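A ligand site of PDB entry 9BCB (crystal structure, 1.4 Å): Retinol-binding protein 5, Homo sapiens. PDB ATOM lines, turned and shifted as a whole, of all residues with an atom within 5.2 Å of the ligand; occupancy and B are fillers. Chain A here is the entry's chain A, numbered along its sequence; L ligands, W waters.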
ATOM      1  N   GLN A  14     -35.620  -6.832 -19.149  1.00  0.00           N
ATOM      2  CA  GLN A  14     -34.831  -5.687 -18.718  1.00  0.00           C
ATOM      3  C   GLN A  14     -34.469  -4.870 -19.956  1.00  0.00           C
ATOM      4  O   GLN A  14     -34.379  -5.393 -21.063  1.00  0.00           O
ATOM      5  CB  GLN A  14     -33.555  -6.095 -17.984  1.00  0.00           C
ATOM      6  CG  GLN A  14     -32.424  -6.556 -18.866  1.00  0.00           C
ATOM      7  CD  GLN A  14     -31.289  -7.184 -18.071  1.00  0.00           C
ATOM      8  OE1 GLN A  14     -31.261  -7.094 -16.838  1.00  0.00           O
ATOM      9  NE2 GLN A  14     -30.357  -7.823 -18.758  1.00  0.00           N
ATOM     10  N   MET A  17     -29.769  -2.269 -19.310  1.00  0.00           N
ATOM     11  CA  MET A  17     -28.747  -2.801 -18.414  1.00  0.00           C
ATOM     12  C   MET A  17     -27.348  -2.457 -18.912  1.00  0.00           C
ATOM     13  O   MET A  17     -26.444  -2.232 -18.095  1.00  0.00           O
ATOM     14  CB  MET A  17     -28.919  -4.322 -18.287  1.00  0.00           C
ATOM     15  CG  MET A  17     -27.908  -5.011 -17.392  1.00  0.00           C
ATOM     16  SD  MET A  17     -27.806  -4.314 -15.727  1.00  0.00           S
ATOM     17  CE  MET A  17     -29.212  -5.100 -14.932  1.00  0.00           C
ATOM     18  N   TYR A  20     -26.429   0.867 -17.293  1.00  0.00           N
ATOM     19  CA  TYR A  20     -26.138   0.765 -15.867  1.00  0.00           C
ATOM     20  C   TYR A  20     -24.793   0.098 -15.623  1.00  0.00           C
ATOM     21  O   TYR A  20     -24.006   0.546 -14.784  1.00  0.00           O
ATOM     22  CB  TYR A  20     -27.291   0.003 -15.188  1.00  0.00           C
ATOM     23  CG  TYR A  20     -27.126  -0.261 -13.709  1.00  0.00           C
ATOM     24  CD1 TYR A  20     -27.334   0.746 -12.778  1.00  0.00           C
ATOM     25  CD2 TYR A  20     -26.814  -1.535 -13.249  1.00  0.00           C
ATOM     26  CE1 TYR A  20     -27.204   0.490 -11.418  1.00  0.00           C
ATOM     27  CE2 TYR A  20     -26.680  -1.791 -11.898  1.00  0.00           C
ATOM     28  CZ  TYR A  20     -26.884  -0.773 -10.987  1.00  0.00           C
ATOM     29  OH  TYR A  20     -26.747  -1.042  -9.647  1.00  0.00           O
ATOM     30  N   LEU A  21     -24.490  -0.970 -16.364  1.00  0.00           N
ATOM     31  CA  LEU A  21     -23.209  -1.650 -16.189  1.00  0.00           C
ATOM     32  C   LEU A  21     -22.043  -0.729 -16.516  1.00  0.00           C
ATOM     33  O   LEU A  21     -21.048  -0.686 -15.785  1.00  0.00           O
ATOM     34  CB  LEU A  21     -23.156  -2.903 -17.068  1.00  0.00           C
ATOM     35  CG  LEU A  21     -24.041  -4.070 -16.669  1.00  0.00           C
ATOM     36  CD1 LEU A  21     -24.279  -4.994 -17.865  1.00  0.00           C
ATOM     37  CD2 LEU A  21     -23.428  -4.835 -15.513  1.00  0.00           C
ATOM     38  N   LEU A  24     -21.346   1.848 -13.771  1.00  0.00           N
ATOM     39  CA  LEU A  24     -20.592   1.280 -12.668  1.00  0.00           C
ATOM     40  C   LEU A  24     -19.167   0.898 -13.051  1.00  0.00           C
ATOM     41  O   LEU A  24     -18.435   0.374 -12.213  1.00  0.00           O
ATOM     42  CB  LEU A  24     -21.319   0.055 -12.092  1.00  0.00           C
ATOM     43  CG  LEU A  24     -22.674   0.306 -11.427  1.00  0.00           C
ATOM     44  CD1 LEU A  24     -23.216  -0.987 -10.844  1.00  0.00           C
ATOM     45  CD2 LEU A  24     -22.574   1.378 -10.354  1.00  0.00           C
ATOM     46  N   ILE A  26     -18.086  -1.408 -15.101  1.00  0.00           N
ATOM     47  CA  ILE A  26     -17.844  -2.826 -15.325  1.00  0.00           C
ATOM     48  C   ILE A  26     -17.196  -3.023 -16.687  1.00  0.00           C
ATOM     49  O   ILE A  26     -17.569  -2.371 -17.676  1.00  0.00           O
ATOM     50  CB  ILE A  26     -19.169  -3.603 -15.223  1.00  0.00           C
ATOM     51  CG1 ILE A  26     -19.855  -3.359 -13.865  1.00  0.00           C
ATOM     52  CG2 ILE A  26     -18.930  -5.094 -15.434  1.00  0.00           C
ATOM     53  CD1 ILE A  26     -18.981  -3.659 -12.669  1.00  0.00           C
ATOM     54  N   VAL A  30     -17.081  -8.537 -18.752  1.00  0.00           N
ATOM     55  CA  VAL A  30     -18.103  -8.897 -17.780  1.00  0.00           C
ATOM     56  C   VAL A  30     -19.478  -8.430 -18.243  1.00  0.00           C
ATOM     57  O   VAL A  30     -20.480  -9.113 -18.019  1.00  0.00           O
ATOM     58  CB  VAL A  30     -17.728  -8.354 -16.398  1.00  0.00           C
ATOM     59  CG1 VAL A  30     -18.802  -8.675 -15.370  1.00  0.00           C
ATOM     60  CG2 VAL A  30     -16.394  -8.943 -15.959  1.00  0.00           C
ATOM     61  N   ILE A  33     -21.039 -10.959 -20.465  1.00  0.00           N
ATOM     62  CA  ILE A  33     -21.600 -12.070 -19.702  1.00  0.00           C
ATOM     63  C   ILE A  33     -22.928 -11.672 -19.074  1.00  0.00           C
ATOM     64  O   ILE A  33     -23.941 -12.367 -19.219  1.00  0.00           O
ATOM     65  CB  ILE A  33     -20.585 -12.555 -18.646  1.00  0.00           C
ATOM     66  CG1 ILE A  33     -19.313 -13.055 -19.325  1.00  0.00           C
ATOM     67  CG2 ILE A  33     -21.203 -13.642 -17.774  1.00  0.00           C
ATOM     68  CD1 ILE A  33     -18.138 -13.279 -18.374  1.00  0.00           C
ATOM     69  N   ALA A  34     -22.959 -10.527 -18.387  1.00  0.00           N
ATOM     70  CA  ALA A  34     -24.144 -10.134 -17.631  1.00  0.00           C
ATOM     71  C   ALA A  34     -25.357  -9.986 -18.531  1.00  0.00           C
ATOM     72  O   ALA A  34     -26.488 -10.304 -18.130  1.00  0.00           O
ATOM     73  CB  ALA A  34     -23.869  -8.824 -16.893  1.00  0.00           C
ATOM     74  N   LEU A  37     -27.550 -13.197 -19.165  1.00  0.00           N
ATOM     75  CA  LEU A  37     -28.196 -13.913 -18.075  1.00  0.00           C
ATOM     76  C   LEU A  37     -29.575 -13.358 -17.772  1.00  0.00           C
ATOM     77  O   LEU A  37     -29.945 -12.251 -18.190  1.00  0.00           O
ATOM     78  CB  LEU A  37     -27.341 -13.862 -16.816  1.00  0.00           C
ATOM     79  CG  LEU A  37     -25.895 -14.337 -16.985  1.00  0.00           C
ATOM     80  CD1 LEU A  37     -25.125 -14.184 -15.680  1.00  0.00           C
ATOM     81  CD2 LEU A  37     -25.864 -15.780 -17.467  1.00  0.00           C
ATOM     82  N   PRO A  39     -31.251 -13.129 -14.337  1.00  0.00           N
ATOM     83  CA  PRO A  39     -31.220 -13.342 -12.877  1.00  0.00           C
ATOM     84  C   PRO A  39     -32.586 -13.170 -12.249  1.00  0.00           C
ATOM     85  O   PRO A  39     -33.381 -12.320 -12.654  1.00  0.00           O
ATOM     86  CB  PRO A  39     -30.244 -12.274 -12.382  1.00  0.00           C
ATOM     87  CG  PRO A  39     -29.505 -11.789 -13.609  1.00  0.00           C
ATOM     88  CD  PRO A  39     -30.496 -11.923 -14.720  1.00  0.00           C
ATOM     89  N   LYS A  41     -35.014 -12.726  -8.589  1.00  0.00           N
ATOM     90  CA  LYS A  41     -35.028 -11.902  -7.387  1.00  0.00           C
ATOM     91  C   LYS A  41     -35.795 -12.642  -6.304  1.00  0.00           C
ATOM     92  O   LYS A  41     -36.931 -13.068  -6.528  1.00  0.00           O
ATOM     93  CB  LYS A  41     -35.689 -10.543  -7.678  1.00  0.00           C
ATOM     94  CG  LYS A  41     -35.408  -9.444  -6.655  1.00  0.00           C
ATOM     95  CD  LYS A  41     -33.965  -8.936  -6.716  1.00  0.00           C
ATOM     96  CE  LYS A  41     -33.579  -8.396  -8.085  1.00  0.00           C
ATOM     97  NZ  LYS A  41     -32.305  -7.617  -8.033  1.00  0.00           N
ATOM     98  N   VAL A  52     -32.552  -9.382   0.342  1.00  0.00           N
ATOM     99  CA  VAL A  52     -32.826  -9.345  -1.093  1.00  0.00           C
ATOM    100  C   VAL A  52     -31.691 -10.072  -1.800  1.00  0.00           C
ATOM    101  O   VAL A  52     -30.524  -9.670  -1.664  1.00  0.00           O
ATOM    102  CB  VAL A  52     -32.980  -7.916  -1.624  1.00  0.00           C
ATOM    103  CG1 VAL A  52     -33.425  -7.953  -3.077  1.00  0.00           C
ATOM    104  CG2 VAL A  52     -33.955  -7.132  -0.784  1.00  0.00           C
ATOM    105  N   THR A  54     -30.202 -11.512  -5.520  1.00  0.00           N
ATOM    106  CA  THR A  54     -30.202 -11.539  -6.981  1.00  0.00           C
ATOM    107  C   THR A  54     -29.454 -12.805  -7.369  1.00  0.00           C
ATOM    108  O   THR A  54     -28.284 -12.979  -7.002  1.00  0.00           O
ATOM    109  CB  THR A  54     -29.511 -10.294  -7.527  1.00  0.00           C
ATOM    110  OG1 THR A  54     -30.135  -9.123  -6.973  1.00  0.00           O
ATOM    111  CG2 THR A  54     -29.620 -10.237  -9.046  1.00  0.00           C
ATOM    112  N   SER A  56     -28.235 -15.798 -10.113  1.00  0.00           N
ATOM    113  CA  SER A  56     -27.930 -16.208 -11.470  1.00  0.00           C
ATOM    114  C   SER A  56     -26.984 -17.398 -11.455  1.00  0.00           C
ATOM    115  O   SER A  56     -26.373 -17.726 -10.432  1.00  0.00           O
ATOM    116  CB  SER A  56     -27.292 -15.067 -12.282  1.00  0.00           C
ATOM    117  OG  SER A  56     -25.898 -15.023 -12.069  1.00  0.00           O
ATOM    118  N   PHE A  58     -24.132 -17.621 -12.862  1.00  0.00           N
ATOM    119  CA  PHE A  58     -22.735 -17.206 -12.765  1.00  0.00           C
ATOM    120  C   PHE A  58     -22.378 -16.675 -11.382  1.00  0.00           C
ATOM    121  O   PHE A  58     -21.294 -16.972 -10.870  1.00  0.00           O
ATOM    122  CB  PHE A  58     -22.440 -16.121 -13.793  1.00  0.00           C
ATOM    123  CG  PHE A  58     -22.047 -16.642 -15.139  1.00  0.00           C
ATOM    124  CD1 PHE A  58     -22.985 -17.265 -15.961  1.00  0.00           C
ATOM    125  CD2 PHE A  58     -20.750 -16.519 -15.589  1.00  0.00           C
ATOM    126  CE1 PHE A  58     -22.609 -17.749 -17.211  1.00  0.00           C
ATOM    127  CE2 PHE A  58     -20.378 -16.990 -16.828  1.00  0.00           C
ATOM    128  CZ  PHE A  58     -21.308 -17.607 -17.646  1.00  0.00           C
ATOM    129  N   ARG A  59     -23.255 -15.868 -10.783  1.00  0.00           N
ATOM    130  CA  ARG A  59     -22.932 -15.206  -9.527  1.00  0.00           C
ATOM    131  C   ARG A  59     -24.223 -14.742  -8.885  1.00  0.00           C
ATOM    132  O   ARG A  59     -25.186 -14.414  -9.569  1.00  0.00           O
ATOM    133  CB  ARG A  59     -21.986 -14.019  -9.769  1.00  0.00           C
ATOM    134  CG  ARG A  59     -21.879 -13.034  -8.610  1.00  0.00           C
ATOM    135  CD  ARG A  59     -20.702 -12.102  -8.829  1.00  0.00           C
ATOM    136  NE  ARG A  59     -19.425 -12.809  -8.703  1.00  0.00           N
ATOM    137  CZ  ARG A  59     -18.231 -12.259  -8.843  1.00  0.00           C
ATOM    138  NH1 ARG A  59     -17.137 -12.992  -8.712  1.00  0.00           N
ATOM    139  NH2 ARG A  59     -18.122 -10.958  -9.128  1.00  0.00           N
ATOM    140  N   ASN A  60     -24.227 -14.737  -7.553  1.00  0.00           N
ATOM    141  CA  ASN A  60     -25.349 -14.245  -6.776  1.00  0.00           C
ATOM    142  C   ASN A  60     -24.889 -13.027  -5.976  1.00  0.00           C
ATOM    143  O   ASN A  60     -23.707 -12.884  -5.669  1.00  0.00           O
ATOM    144  CB  ASN A  60     -25.849 -15.310  -5.795  1.00  0.00           C
ATOM    145  CG  ASN A  60     -26.232 -16.596  -6.485  1.00  0.00           C
ATOM    146  OD1 ASN A  60     -26.991 -16.595  -7.450  1.00  0.00           O
ATOM    147  ND2 ASN A  60     -25.699 -17.708  -5.995  1.00  0.00           N
ATOM    148  N   TYR A  61     -25.844 -12.156  -5.647  1.00  0.00           N
ATOM    149  CA  TYR A  61     -25.555 -11.028  -4.775  1.00  0.00           C
ATOM    150  C   TYR A  61     -26.677 -10.889  -3.765  1.00  0.00           C
ATOM    151  O   TYR A  61     -27.852 -10.848  -4.150  1.00  0.00           O
ATOM    152  CB  TYR A  61     -25.412  -9.716  -5.561  1.00  0.00           C
ATOM    153  CG  TYR A  61     -25.178  -8.529  -4.655  1.00  0.00           C
ATOM    154  CD1 TYR A  61     -23.971  -8.385  -3.962  1.00  0.00           C
ATOM    155  CD2 TYR A  61     -26.158  -7.571  -4.453  1.00  0.00           C
ATOM    156  CE1 TYR A  61     -23.755  -7.316  -3.123  1.00  0.00           C
ATOM    157  CE2 TYR A  61     -25.960  -6.501  -3.612  1.00  0.00           C
ATOM    158  CZ  TYR A  61     -24.748  -6.373  -2.952  1.00  0.00           C
ATOM    159  OH  TYR A  61     -24.537  -5.305  -2.104  1.00  0.00           O
ATOM    160  N   VAL A  63     -27.996  -8.735  -0.206  1.00  0.00           N
ATOM    161  CA  VAL A  63     -27.890  -7.592   0.687  1.00  0.00           C
ATOM    162  C   VAL A  63     -28.984  -7.736   1.736  1.00  0.00           C
ATOM    163  O   VAL A  63     -30.047  -8.307   1.477  1.00  0.00           O
ATOM    164  CB  VAL A  63     -28.016  -6.252  -0.077  1.00  0.00           C
ATOM    165  CG1 VAL A  63     -29.422  -6.081  -0.644  1.00  0.00           C
ATOM    166  CG2 VAL A  63     -27.652  -5.090   0.815  1.00  0.00           C
ATOM    167  N   GLU A  73     -22.822  -1.048   2.636  1.00  0.00           N
ATOM    168  CA  GLU A  73     -23.135  -2.121   1.702  1.00  0.00           C
ATOM    169  C   GLU A  73     -21.872  -2.563   0.980  1.00  0.00           C
ATOM    170  O   GLU A  73     -21.172  -1.749   0.379  1.00  0.00           O
ATOM    171  CB  GLU A  73     -24.181  -1.661   0.684  1.00  0.00           C
ATOM    172  CG  GLU A  73     -24.687  -2.815  -0.178  1.00  0.00           C
ATOM    173  CD  GLU A  73     -25.742  -2.420  -1.184  1.00  0.00           C
ATOM    174  OE1 GLU A  73     -26.126  -1.232  -1.238  1.00  0.00           O
ATOM    175  OE2 GLU A  73     -26.190  -3.308  -1.942  1.00  0.00           O
ATOM    176  N   SER A  77     -18.171  -7.445  -4.777  1.00  0.00           N
ATOM    177  CA  SER A  77     -18.446  -8.511  -5.736  1.00  0.00           C
ATOM    178  C   SER A  77     -19.248  -8.024  -6.930  1.00  0.00           C
ATOM    179  O   SER A  77     -19.481  -8.804  -7.859  1.00  0.00           O
ATOM    180  CB  SER A  77     -19.184  -9.652  -5.044  1.00  0.00           C
ATOM    181  OG  SER A  77     -20.553  -9.326  -4.841  1.00  0.00           O
ATOM    182  N   VAL A  78     -19.679  -6.759  -6.944  1.00  0.00           N
ATOM    183  CA  VAL A  78     -20.446  -6.202  -8.056  1.00  0.00           C
ATOM    184  C   VAL A  78     -19.541  -5.300  -8.880  1.00  0.00           C
ATOM    185  O   VAL A  78     -19.207  -5.602 -10.030  1.00  0.00           O
ATOM    186  CB  VAL A  78     -21.685  -5.457  -7.536  1.00  0.00           C
ATOM    187  CG1 VAL A  78     -22.453  -4.782  -8.669  1.00  0.00           C
ATOM    188  CG2 VAL A  78     -22.592  -6.432  -6.799  1.00  0.00           C
ATOM    189  N   ASP A  79     -19.133  -4.173  -8.297  1.00  0.00           N
ATOM    190  CA  ASP A  79     -18.290  -3.207  -8.988  1.00  0.00           C
ATOM    191  C   ASP A  79     -17.030  -2.853  -8.201  1.00  0.00           C
ATOM    192  O   ASP A  79     -16.375  -1.854  -8.533  1.00  0.00           O
ATOM    193  CB  ASP A  79     -19.085  -1.938  -9.313  1.00  0.00           C
ATOM    194  CG  ASP A  79     -19.459  -1.158  -8.075  1.00  0.00           C
ATOM    195  OD1 ASP A  79     -19.726  -1.781  -7.026  1.00  0.00           O
ATOM    196  OD2 ASP A  79     -19.503   0.088  -8.151  1.00  0.00           O
ATOM    197  N   TRP A 107     -31.667   2.229  -6.390  1.00  0.00           N
ATOM    198  CA  TRP A 107     -32.704   1.471  -7.074  1.00  0.00           C
ATOM    199  C   TRP A 107     -34.048   1.706  -6.405  1.00  0.00           C
ATOM    200  O   TRP A 107     -34.138   2.275  -5.315  1.00  0.00           O
ATOM    201  CB  TRP A 107     -32.356  -0.023  -7.151  1.00  0.00           C
ATOM    202  CG  TRP A 107     -31.900  -0.666  -5.858  1.00  0.00           C
ATOM    203  CD1 TRP A 107     -30.619  -0.946  -5.480  1.00  0.00           C
ATOM    204  CD2 TRP A 107     -32.738  -1.124  -4.792  1.00  0.00           C
ATOM    205  NE1 TRP A 107     -30.599  -1.560  -4.250  1.00  0.00           N
ATOM    206  CE2 TRP A 107     -31.896  -1.683  -3.800  1.00  0.00           C
ATOM    207  CE3 TRP A 107     -34.115  -1.124  -4.573  1.00  0.00           C
ATOM    208  CZ2 TRP A 107     -32.381  -2.214  -2.616  1.00  0.00           C
ATOM    209  CZ3 TRP A 107     -34.601  -1.668  -3.392  1.00  0.00           C
ATOM    210  CH2 TRP A 107     -33.738  -2.196  -2.431  1.00  0.00           C
ATOM    211  N   HIS A 109     -37.808  -0.597  -5.993  1.00  0.00           N
ATOM    212  CA  HIS A 109     -38.836  -1.604  -6.248  1.00  0.00           C
ATOM    213  C   HIS A 109     -40.255  -1.097  -6.028  1.00  0.00           C
ATOM    214  O   HIS A 109     -40.512  -0.263  -5.153  1.00  0.00           O
ATOM    215  CB  HIS A 109     -38.724  -2.907  -5.443  1.00  0.00           C
ATOM    216  CG  HIS A 109     -37.597  -3.808  -5.822  1.00  0.00           C
ATOM    217  ND1 HIS A 109     -37.669  -4.599  -6.952  1.00  0.00           N
ATOM    218  CD2 HIS A 109     -36.480  -4.195  -5.167  1.00  0.00           C
ATOM    219  CE1 HIS A 109     -36.584  -5.351  -7.020  1.00  0.00           C
ATOM    220  NE2 HIS A 109     -35.857  -5.136  -5.945  1.00  0.00           N
ATOM    221  N   LEU A 118     -38.286  -3.146 -10.994  1.00  0.00           N
ATOM    222  CA  LEU A 118     -37.036  -2.668 -10.435  1.00  0.00           C
ATOM    223  C   LEU A 118     -36.444  -1.640 -11.372  1.00  0.00           C
ATOM    224  O   LEU A 118     -36.233  -1.924 -12.560  1.00  0.00           O
ATOM    225  CB  LEU A 118     -36.036  -3.804 -10.205  1.00  0.00           C
ATOM    226  CG  LEU A 118     -34.678  -3.387  -9.642  1.00  0.00           C
ATOM    227  CD1 LEU A 118     -34.826  -2.618  -8.334  1.00  0.00           C
ATOM    228  CD2 LEU A 118     -33.770  -4.596  -9.445  1.00  0.00           C
ATOM    229  N   LEU A 120     -33.054   0.681 -11.724  1.00  0.00           N
ATOM    230  CA  LEU A 120     -31.672   0.753 -11.266  1.00  0.00           C
ATOM    231  C   LEU A 120     -31.046   2.003 -11.856  1.00  0.00           C
ATOM    232  O   LEU A 120     -31.188   2.251 -13.065  1.00  0.00           O
ATOM    233  CB  LEU A 120     -30.897  -0.462 -11.770  1.00  0.00           C
ATOM    234  CG  LEU A 120     -31.218  -1.830 -11.160  1.00  0.00           C
ATOM    235  CD1 LEU A 120     -30.899  -2.906 -12.178  1.00  0.00           C
ATOM    236  CD2 LEU A 120     -30.444  -2.068  -9.886  1.00  0.00           C
HETATM  237  C1  LIG L   1     -31.310  -4.311  -6.252  1.00  0.00           C
HETATM  238  C2  LIG L   1     -32.220  -4.906  -5.182  1.00  0.00           C
HETATM  239  C3  LIG L   1     -31.311  -5.553  -4.131  1.00  0.00           C
HETATM  240  C4  LIG L   1     -29.507  -5.010  -7.573  1.00  0.00           C
HETATM  241  C5  LIG L   1     -24.271  -4.833 -12.128  1.00  0.00           C
HETATM  242  C6  LIG L   1     -27.023  -8.171 -14.306  1.00  0.00           C
HETATM  243  C7  LIG L   1     -21.785 -12.387 -13.788  1.00  0.00           C
HETATM  244  C8  LIG L   1     -19.480  -8.681 -11.629  1.00  0.00           C
HETATM  245  C9  LIG L   1     -24.603  -8.274 -13.312  1.00  0.00           C
HETATM  246  C10 LIG L   1     -25.813  -7.561 -13.605  1.00  0.00           C
HETATM  247  C11 LIG L   1     -25.720  -6.416 -13.217  1.00  0.00           C
HETATM  248  C12 LIG L   1     -20.627  -9.429 -12.312  1.00  0.00           C
HETATM  249  C13 LIG L   1     -24.649  -6.201 -12.710  1.00  0.00           C
HETATM  250  C14 LIG L   1     -20.539 -10.597 -12.702  1.00  0.00           C
HETATM  251  C15 LIG L   1     -21.599 -10.979 -13.209  1.00  0.00           C
HETATM  252  C16 LIG L   1     -24.073  -9.771 -13.612  1.00  0.00           C
HETATM  253  C17 LIG L   1     -22.614 -10.026 -13.230  1.00  0.00           C
HETATM  254  C18 LIG L   1     -29.075  -5.926  -8.717  1.00  0.00           C
HETATM  255  B1  LIG L   1     -22.457  -7.484 -12.213  1.00  0.00           B
HETATM  256  C19 LIG L   1     -25.050 -10.923 -13.846  1.00  0.00           C
HETATM  257  C20 LIG L   1     -27.736  -5.515  -9.329  1.00  0.00           C
HETATM  258  C21 LIG L   1     -26.530  -6.074  -8.556  1.00  0.00           C
HETATM  259  C22 LIG L   1     -26.524  -7.600  -8.451  1.00  0.00           C
HETATM  260  C23 LIG L   1     -25.739  -8.255  -9.589  1.00  0.00           C
HETATM  261  C24 LIG L   1     -25.777  -9.764  -9.391  1.00  0.00           C
HETATM  262  C25 LIG L   1     -24.970 -10.456 -10.488  1.00  0.00           C
HETATM  263  C26 LIG L   1     -25.937 -11.029 -11.523  1.00  0.00           C
HETATM  264  C27 LIG L   1     -25.141 -11.783 -12.587  1.00  0.00           C
HETATM  265  F1  LIG L   1     -21.495  -6.321 -12.900  1.00  0.00           F
HETATM  266  F2  LIG L   1     -22.464  -7.401 -10.557  1.00  0.00           F
HETATM  267  N1  LIG L   1     -21.833  -8.844 -12.528  1.00  0.00           N
HETATM  268  N2  LIG L   1     -23.807  -7.257 -12.666  1.00  0.00           N
HETATM  269  O1  LIG L   1     -29.961  -5.584  -4.548  1.00  0.00           O
HETATM  270  O2  LIG L   1     -28.926  -3.995  -7.331  1.00  0.00           O
HETATM  271  O3  LIG L   1     -30.622  -5.378  -6.819  1.00  0.00           O
HETATM  272  O4  LIG L   1     -33.062  -5.850  -5.809  1.00  0.00           O
HETATM  273  O   HOH W   1     -29.372  -7.918 -12.389  1.00  0.00           O
HETATM  274  O   HOH W   2     -29.630  -8.612  -4.330  1.00  0.00           O
HETATM  275  O   HOH W   3     -31.483  -7.129 -10.641  1.00  0.00           O
HETATM  276  O   HOH W   4     -29.970  -8.734 -15.192  1.00  0.00           O
HETATM  277  O   HOH W   5     -28.383  -3.483  -3.539  1.00  0.00           O
HETATM  278  O   HOH W   6     -21.960  -9.410  -8.883  1.00  0.00           O
HETATM  279  O   HOH W   7     -26.934  -2.763  -6.025  1.00  0.00           O
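Merely in contact with the ligand: Val 78, Leu 21, Ser 56, Val 52, Ala 34, Trp 107, Ile 26, Leu 120, Val 30, Arg 59, Leu 37, Tyr 61, Ser 77, Thr 54, Phe 58, Met 17, Tyr 20, Leu 118 and Val 63. Within 4 Å of the ligand: Met 17, Tyr 20, Leu 21, Ile 26, Val 30, Ala 34, Leu 37, Lys 41, Val 52, Thr 54, Ser 56, Phe 58, Arg 59, Tyr 61, Val 63, Ser 77, Val 78, Trp 107, His 109, Leu 118 and Leu 120. The nearest printed residue that does not touch the ligand is Leu 24 (4.2 Å).
NE2 of His 109 is in hydrogen-bond range of O4 of the ligand, at 2.9 Å. NZ of Lys 41 lies within hydrogen-bond range of O4 of the ligand, 2.9 Å away.
Water W5 lies within hydrogen-bond range of OE2 of Glu 73 (2.7 Å), O1 of the ligand (2.8 Å) and NE1 of Trp 107 (3.0 Å). Water W2 lies within hydrogen-bond range of OG1 of Thr 54 (2.7 Å), O of Tyr 61 (2.9 Å), O of Val 52 (3.0 Å) and O1 of the ligand (3.1 Å).
The backbone NH of Ser 56 is in hydrogen-bond range of the side-chain amide oxygen of Asn 60 (3.0 Å). The side-chain hydroxyl (OG) of Ser 56 lies close to the backbone NH (N) of Phe 58, at 3.2 Å. The backbone carbonyl oxygen of Ser 77 lies within hydrogen-bond range of the guanidinium group of Arg 59 (2.8 Å). OG of Ser 56 sits at hydrogen-bond distance from O of Arg 59 (2.7 Å). The backbone NH (N) of Val 52 is in hydrogen-bond range of the backbone carbonyl oxygen (O) of Val 63, 3.0 Å away. The backbone NH (N) of Ile 26 is in hydrogen-bond range of the backbone carbonyl oxygen (O) of Leu 21, 3.1 Å away. The side-chain hydroxyl of Thr 54 sits at hydrogen-bond distance from the side-chain amino group of Lys 41 (2.8 Å). N of Thr 54 is in hydrogen-bond range of O of Tyr 61 (2.8 Å).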
